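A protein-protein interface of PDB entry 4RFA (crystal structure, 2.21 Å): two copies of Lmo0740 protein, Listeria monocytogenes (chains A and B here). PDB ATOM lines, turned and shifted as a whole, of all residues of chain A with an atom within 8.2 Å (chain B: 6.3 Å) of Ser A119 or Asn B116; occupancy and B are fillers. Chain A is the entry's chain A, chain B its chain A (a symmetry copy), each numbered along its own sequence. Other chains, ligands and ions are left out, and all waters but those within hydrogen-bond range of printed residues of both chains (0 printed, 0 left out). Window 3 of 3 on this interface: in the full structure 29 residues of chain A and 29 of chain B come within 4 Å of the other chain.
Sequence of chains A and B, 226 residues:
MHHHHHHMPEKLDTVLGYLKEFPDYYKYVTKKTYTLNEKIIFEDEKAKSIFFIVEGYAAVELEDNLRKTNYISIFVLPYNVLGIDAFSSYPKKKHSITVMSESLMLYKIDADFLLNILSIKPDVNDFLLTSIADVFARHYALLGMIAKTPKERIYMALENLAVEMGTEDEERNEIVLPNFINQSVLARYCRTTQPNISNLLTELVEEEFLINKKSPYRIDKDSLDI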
ATOM      1  N   PHE A 113     -23.190   9.917 -18.315  1.00  0.00           N
ATOM      2  CA  PHE A 113     -22.360   9.524 -17.170  1.00  0.00           C
ATOM      3  C   PHE A 113     -22.713  10.337 -15.953  1.00  0.00           C
ATOM      4  O   PHE A 113     -23.060   9.818 -14.915  1.00  0.00           O
ATOM      5  CB  PHE A 113     -20.879   9.763 -17.486  1.00  0.00           C
ATOM      6  CG  PHE A 113     -19.914   9.379 -16.376  1.00  0.00           C
ATOM      7  CD1 PHE A 113     -19.877   8.073 -15.859  1.00  0.00           C
ATOM      8  CD2 PHE A 113     -18.952  10.284 -15.932  1.00  0.00           C
ATOM      9  CE1 PHE A 113     -18.949   7.721 -14.877  1.00  0.00           C
ATOM     10  CE2 PHE A 113     -18.017   9.931 -14.964  1.00  0.00           C
ATOM     11  CZ  PHE A 113     -18.011   8.647 -14.434  1.00  0.00           C
ATOM     12  N   LEU A 114     -22.604  11.639 -16.096  1.00  0.00           N
ATOM     13  CA  LEU A 114     -22.806  12.528 -14.974  1.00  0.00           C
ATOM     14  C   LEU A 114     -24.226  12.339 -14.467  1.00  0.00           C
ATOM     15  O   LEU A 114     -24.432  12.211 -13.253  1.00  0.00           O
ATOM     16  CB  LEU A 114     -22.578  13.997 -15.389  1.00  0.00           C
ATOM     17  CG  LEU A 114     -22.888  14.977 -14.257  1.00  0.00           C
ATOM     18  CD1 LEU A 114     -22.023  14.721 -13.029  1.00  0.00           C
ATOM     19  CD2 LEU A 114     -22.742  16.418 -14.737  1.00  0.00           C
ATOM     20  N   LEU A 115     -25.184  12.290 -15.394  1.00  0.00           N
ATOM     21  CA  LEU A 115     -26.615  12.075 -15.038  1.00  0.00           C
ATOM     22  C   LEU A 115     -26.913  10.740 -14.361  1.00  0.00           C
ATOM     23  O   LEU A 115     -28.017  10.552 -13.831  1.00  0.00           O
ATOM     24  CB  LEU A 115     -27.536  12.224 -16.272  1.00  0.00           C
ATOM     25  N   ASN A 116     -25.954   9.813 -14.403  1.00  0.00           N
ATOM     26  CA  ASN A 116     -26.102   8.516 -13.738  1.00  0.00           C
ATOM     27  C   ASN A 116     -25.529   8.474 -12.333  1.00  0.00           C
ATOM     28  O   ASN A 116     -25.975   7.682 -11.503  1.00  0.00           O
ATOM     29  CB  ASN A 116     -25.424   7.412 -14.560  1.00  0.00           C
ATOM     30  CG  ASN A 116     -26.332   6.839 -15.617  1.00  0.00           C
ATOM     31  OD1 ASN A 116     -27.533   6.683 -15.391  1.00  0.00           O
ATOM     32  ND2 ASN A 116     -25.766   6.501 -16.771  1.00  0.00           N
ATOM     33  N   ILE A 117     -24.535   9.308 -12.065  1.00  0.00           N
ATOM     34  CA  ILE A 117     -23.789   9.180 -10.815  1.00  0.00           C
ATOM     35  C   ILE A 117     -24.303  10.158  -9.777  1.00  0.00           C
ATOM     36  O   ILE A 117     -23.686  10.357  -8.731  1.00  0.00           O
ATOM     37  CB  ILE A 117     -22.280   9.318 -11.053  1.00  0.00           C
ATOM     38  CG1 ILE A 117     -21.951  10.612 -11.767  1.00  0.00           C
ATOM     39  CG2 ILE A 117     -21.815   8.172 -11.938  1.00  0.00           C
ATOM     40  CD1 ILE A 117     -20.553  10.663 -12.323  1.00  0.00           C
ATOM     41  N   LEU A 118     -25.465  10.734 -10.057  1.00  0.00           N
ATOM     42  CA  LEU A 118     -26.059  11.698  -9.162  1.00  0.00           C
ATOM     43  C   LEU A 118     -26.638  10.964  -7.963  1.00  0.00           C
ATOM     44  O   LEU A 118     -26.177  11.138  -6.826  1.00  0.00           O
ATOM     45  CB  LEU A 118     -27.127  12.512  -9.908  1.00  0.00           C
ATOM     46  CG  LEU A 118     -26.583  13.233 -11.155  1.00  0.00           C
ATOM     47  CD1 LEU A 118     -27.605  14.153 -11.814  1.00  0.00           C
ATOM     48  CD2 LEU A 118     -25.323  14.009 -10.798  1.00  0.00           C
ATOM     49  N   SER A 119     -27.616  10.106  -8.235  1.00  0.00           N
ATOM     50  CA  SER A 119     -28.259   9.309  -7.204  1.00  0.00           C
ATOM     51  C   SER A 119     -27.188   8.652  -6.345  1.00  0.00           C
ATOM     52  O   SER A 119     -27.226   8.730  -5.123  1.00  0.00           O
ATOM     53  CB  SER A 119     -29.151   8.234  -7.840  1.00  0.00           C
ATOM     54  OG  SER A 119     -29.638   8.650  -9.108  1.00  0.00           O
ATOM     55  N   ILE A 120     -26.210   8.051  -7.009  1.00  0.00           N
ATOM     56  CA  ILE A 120     -25.212   7.217  -6.345  1.00  0.00           C
ATOM     57  C   ILE A 120     -24.363   7.970  -5.318  1.00  0.00           C
ATOM     58  O   ILE A 120     -23.953   7.400  -4.300  1.00  0.00           O
ATOM     59  CB  ILE A 120     -24.265   6.576  -7.390  1.00  0.00           C
ATOM     60  CG1 ILE A 120     -25.042   5.612  -8.295  1.00  0.00           C
ATOM     61  CG2 ILE A 120     -23.112   5.843  -6.712  1.00  0.00           C
ATOM     62  CD1 ILE A 120     -24.460   5.464  -9.684  1.00  0.00           C
ATOM     63  N   LYS A 121     -24.086   9.239  -5.594  1.00  0.00           N
ATOM     64  CA  LYS A 121     -23.040   9.946  -4.882  1.00  0.00           C
ATOM     65  C   LYS A 121     -23.679  10.859  -3.843  1.00  0.00           C
ATOM     66  O   LYS A 121     -24.521  11.695  -4.194  1.00  0.00           O
ATOM     67  CB  LYS A 121     -22.177  10.719  -5.877  1.00  0.00           C
ATOM     68  CG  LYS A 121     -21.571   9.842  -6.976  1.00  0.00           C
ATOM     69  CD  LYS A 121     -20.379   9.044  -6.484  1.00  0.00           C
ATOM     70  N   PRO A 122     -23.293  10.691  -2.558  1.00  0.00           N
ATOM     71  CA  PRO A 122     -23.930  11.402  -1.426  1.00  0.00           C
ATOM     72  C   PRO A 122     -23.586  12.897  -1.275  1.00  0.00           C
ATOM     73  O   PRO A 122     -23.977  13.515  -0.287  1.00  0.00           O
ATOM     74  CB  PRO A 122     -23.476  10.598  -0.197  1.00  0.00           C
ATOM     75  CG  PRO A 122     -22.214   9.919  -0.610  1.00  0.00           C
ATOM     76  CD  PRO A 122     -22.267   9.728  -2.101  1.00  0.00           C
ATOM     77  N   ASP A 123     -22.844  13.458  -2.229  1.00  0.00           N
ATOM     78  CA  ASP A 123     -22.865  14.895  -2.502  1.00  0.00           C
ATOM     79  C   ASP A 123     -24.023  15.106  -3.465  1.00  0.00           C
ATOM     80  O   ASP A 123     -23.879  15.651  -4.573  1.00  0.00           O
ATOM     81  CB  ASP A 123     -21.554  15.309  -3.146  1.00  0.00           C
ATOM     82  CG  ASP A 123     -21.597  16.697  -3.689  1.00  0.00           C
ATOM     83  OD1 ASP A 123     -22.613  17.409  -3.489  1.00  0.00           O
ATOM     84  OD2 ASP A 123     -20.608  17.073  -4.338  1.00  0.00           O
ATOM     85  N   VAL A 124     -25.188  14.690  -2.991  1.00  0.00           N
ATOM     86  CA  VAL A 124     -26.229  14.145  -3.849  1.00  0.00           C
ATOM     87  C   VAL A 124     -26.841  15.177  -4.762  1.00  0.00           C
ATOM     88  O   VAL A 124     -27.860  15.786  -4.434  1.00  0.00           O
ATOM     89  CB  VAL A 124     -27.342  13.410  -3.037  1.00  0.00           C
ATOM     90  CG1 VAL A 124     -28.133  14.372  -2.137  1.00  0.00           C
ATOM     91  CG2 VAL A 124     -28.272  12.634  -3.975  1.00  0.00           C
ATOM     92  N   ASN A 125     -26.210  15.373  -5.917  1.00  0.00           N
ATOM     93  CA  ASN A 125     -26.792  16.178  -6.976  1.00  0.00           C
ATOM     94  C   ASN A 125     -26.923  17.622  -6.516  1.00  0.00           C
ATOM     95  O   ASN A 125     -26.995  18.536  -7.340  1.00  0.00           O
ATOM     96  CB  ASN A 125     -28.163  15.604  -7.359  1.00  0.00           C
ATOM     97  CG  ASN A 125     -28.658  16.088  -8.707  1.00  0.00           C
ATOM     98  OD1 ASN A 125     -27.907  16.664  -9.499  1.00  0.00           O
ATOM     99  ND2 ASN A 125     -29.942  15.846  -8.976  1.00  0.00           N
ATOM    100  N   ALA B 111     -37.094  16.883  -3.500  1.00  0.00           N
ATOM    101  CA  ALA B 111     -35.934  16.987  -4.355  1.00  0.00           C
ATOM    102  C   ALA B 111     -34.969  15.792  -4.213  1.00  0.00           C
ATOM    103  O   ALA B 111     -34.442  15.252  -5.211  1.00  0.00           O
ATOM    104  CB  ALA B 111     -35.214  18.291  -4.023  1.00  0.00           C
ATOM    105  N   ASP B 112     -34.729  15.360  -2.985  1.00  0.00           N
ATOM    106  CA  ASP B 112     -33.966  14.097  -2.790  1.00  0.00           C
ATOM    107  C   ASP B 112     -34.546  12.913  -3.604  1.00  0.00           C
ATOM    108  O   ASP B 112     -33.795  12.224  -4.324  1.00  0.00           O
ATOM    109  CB  ASP B 112     -33.880  13.720  -1.306  1.00  0.00           C
ATOM    110  CG  ASP B 112     -32.565  14.155  -0.663  1.00  0.00           C
ATOM    111  OD1 ASP B 112     -32.159  15.328  -0.820  1.00  0.00           O
ATOM    112  OD2 ASP B 112     -31.933  13.305   0.006  1.00  0.00           O
ATOM    113  N   PHE B 113     -35.872  12.719  -3.498  1.00  0.00           N
ATOM    114  CA  PHE B 113     -36.601  11.723  -4.293  1.00  0.00           C
ATOM    115  C   PHE B 113     -36.320  11.907  -5.761  1.00  0.00           C
ATOM    116  O   PHE B 113     -35.870  11.014  -6.443  1.00  0.00           O
ATOM    117  CB  PHE B 113     -38.110  11.878  -4.076  1.00  0.00           C
ATOM    118  CG  PHE B 113     -38.975  10.888  -4.840  1.00  0.00           C
ATOM    119  CD1 PHE B 113     -38.814   9.502  -4.679  1.00  0.00           C
ATOM    120  CD2 PHE B 113     -40.036  11.336  -5.625  1.00  0.00           C
ATOM    121  CE1 PHE B 113     -39.651   8.606  -5.347  1.00  0.00           C
ATOM    122  CE2 PHE B 113     -40.879  10.444  -6.279  1.00  0.00           C
ATOM    123  CZ  PHE B 113     -40.691   9.075  -6.141  1.00  0.00           C
ATOM    124  N   LEU B 114     -36.611  13.094  -6.244  1.00  0.00           N
ATOM    125  CA  LEU B 114     -36.495  13.369  -7.659  1.00  0.00           C
ATOM    126  C   LEU B 114     -35.046  13.159  -8.065  1.00  0.00           C
ATOM    127  O   LEU B 114     -34.782  12.503  -9.083  1.00  0.00           O
ATOM    128  CB  LEU B 114     -36.936  14.812  -7.977  1.00  0.00           C
ATOM    129  CG  LEU B 114     -36.724  15.176  -9.447  1.00  0.00           C
ATOM    130  CD1 LEU B 114     -37.503  14.255 -10.379  1.00  0.00           C
ATOM    131  CD2 LEU B 114     -37.083  16.637  -9.698  1.00  0.00           C
ATOM    132  N   LEU B 115     -34.123  13.684  -7.258  1.00  0.00           N
ATOM    133  CA  LEU B 115     -32.664  13.525  -7.520  1.00  0.00           C
ATOM    134  C   LEU B 115     -32.162  12.083  -7.499  1.00  0.00           C
ATOM    135  O   LEU B 115     -31.026  11.822  -7.915  1.00  0.00           O
ATOM    136  CB  LEU B 115     -31.815  14.362  -6.535  1.00  0.00           C
ATOM    137  N   ASN B 116     -32.986  11.165  -6.991  1.00  0.00           N
ATOM    138  CA  ASN B 116     -32.640   9.741  -6.972  1.00  0.00           C
ATOM    139  C   ASN B 116     -33.152   8.964  -8.171  1.00  0.00           C
ATOM    140  O   ASN B 116     -32.574   7.944  -8.544  1.00  0.00           O
ATOM    141  CB  ASN B 116     -33.188   9.073  -5.703  1.00  0.00           C
ATOM    142  CG  ASN B 116     -32.246   9.197  -4.533  1.00  0.00           C
ATOM    143  OD1 ASN B 116     -31.029   9.118  -4.702  1.00  0.00           O
ATOM    144  ND2 ASN B 116     -32.801   9.368  -3.338  1.00  0.00           N
ATOM    145  N   ILE B 117     -34.242   9.428  -8.766  1.00  0.00           N
ATOM    146  CA  ILE B 117     -34.919   8.625  -9.781  1.00  0.00           C
ATOM    147  C   ILE B 117     -34.509   9.059 -11.175  1.00  0.00           C
ATOM    148  O   ILE B 117     -35.110   8.655 -12.169  1.00  0.00           O
ATOM    149  CB  ILE B 117     -36.440   8.652  -9.585  1.00  0.00           C
ATOM    150  CG1 ILE B 117     -36.968  10.071  -9.553  1.00  0.00           C
ATOM    151  CG2 ILE B 117     -36.775   8.006  -8.249  1.00  0.00           C
ATOM    152  CD1 ILE B 117     -38.378  10.186  -9.039  1.00  0.00           C
ATOM    153  N   LEU B 118     -33.447   9.852 -11.239  1.00  0.00           N
ATOM    154  CA  LEU B 118     -32.960  10.352 -12.503  1.00  0.00           C
ATOM    155  C   LEU B 118     -32.245   9.226 -13.234  1.00  0.00           C
ATOM    156  O   LEU B 118     -32.686   8.780 -14.303  1.00  0.00           O
ATOM    157  CB  LEU B 118     -32.040  11.559 -12.266  1.00  0.00           C
ATOM    158  CG  LEU B 118     -32.720  12.700 -11.488  1.00  0.00           C
ATOM    159  CD1 LEU B 118     -31.857  13.952 -11.375  1.00  0.00           C
ATOM    160  CD2 LEU B 118     -34.061  13.036 -12.124  1.00  0.00           C
ATOM    161  N   SER B 119     -31.169   8.742 -12.624  1.00  0.00           N
ATOM    162  CA  SER B 119     -30.387   7.649 -13.178  1.00  0.00           C
ATOM    163  C   SER B 119     -31.329   6.525 -13.589  1.00  0.00           C
ATOM    164  O   SER B 119     -31.259   6.023 -14.705  1.00  0.00           O
ATOM    165  CB  SER B 119     -29.379   7.134 -12.143  1.00  0.00           C
ATOM    166  OG  SER B 119     -28.998   8.161 -11.238  1.00  0.00           O
ATOM    167  N   ILE B 120     -32.238   6.180 -12.687  1.00  0.00           N
ATOM    168  CA  ILE B 120     -33.088   5.004 -12.845  1.00  0.00           C
ATOM    169  C   ILE B 120     -33.996   5.060 -14.077  1.00  0.00           C
ATOM    170  O   ILE B 120     -34.288   4.028 -14.690  1.00  0.00           O
ATOM    171  CB  ILE B 120     -33.974   4.808 -11.590  1.00  0.00           C
ATOM    172  CG1 ILE B 120     -33.103   4.501 -10.364  1.00  0.00           C
ATOM    173  CG2 ILE B 120     -34.992   3.693 -11.802  1.00  0.00           C
ATOM    174  CD1 ILE B 120     -33.707   4.947  -9.050  1.00  0.00           C
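O of Asn A116 sits at hydrogen-bond distance from OG of Ser B119 (3.1 Å).
The backbone carbonyl oxygen (O) of Asn B116 sits at hydrogen-bond distance from the side-chain hydroxyl (OG) of Ser A119 (3.1 Å).
The side-chain hydroxyl (OG) of Ser A119 lies close to the side-chain hydroxyl (OG) of Ser B119 (2.3 Å).
Leu A115 touches Ser B119, and with the chains exchanged Ser A119 touches Leu B115.
Asn A116 touches Ser B119, and with the chains exchanged Ser A119 touches Asn B116.
Ser A119 touches its own counterpart, Ser B119.
Positions printed for both chains: 113, 114, 115, 116, 117, 118, 119 and 120.
Of chain B, only Leu B115 (3.7 Å), Asn B116 (3.1 Å) and Ser B119 (2.3 Å) come within 4 Å of Ser A119.
Printed residues of chain B within 4 Å of Asn A116: Ser B119.
Of the printed residues of chain A, Ser B119 touches Leu A115, Asn A116 and Ser A119.
Of the printed residues of chain B, Leu A115 touches Ser B119 (3.7 Å).
Of the printed residues of chain B, Asn A125 touches Leu B115 (3.4 Å) and Leu B118 (3.6 Å).
Of the printed residues of chain A, Leu B118 touches Asn A125 (3.6 Å).
Ala B111 touches none of the printed residues of chain A.
The nearest residue of chain A that does not touch Asn B116 is Val A124 (4.5 Å).
Among the printed residues, pairs that only touch across the chains: Leu A115 with Ser B119 (3.7 Å), Ser A119 with Leu B115 (3.7 Å), Asn A125 with Leu B115 (3.4 Å) and Asn A125 with Leu B118 (3.6 Å).
Of the 13 printed residues of chain A, 4 touch a printed residue of chain B.
Printed residues of chain A that touch a printed residue of chain B: Leu A115, Asn A116, Ser A119 and Asn A125.
Hydrophobic or aromatic side chains of chain B that line the printed part of chain A: Leu B115 and Leu B118.
Among the printed residues, no Asp or Glu carboxylate lies within 4 Å of a Lys or Arg side-chain nitrogen of the other chain.
The backbone carbonyl oxygen of Asp B112 lies within hydrogen-bond range of the side-chain amide nitrogen of Asn B116 (3.2 Å).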
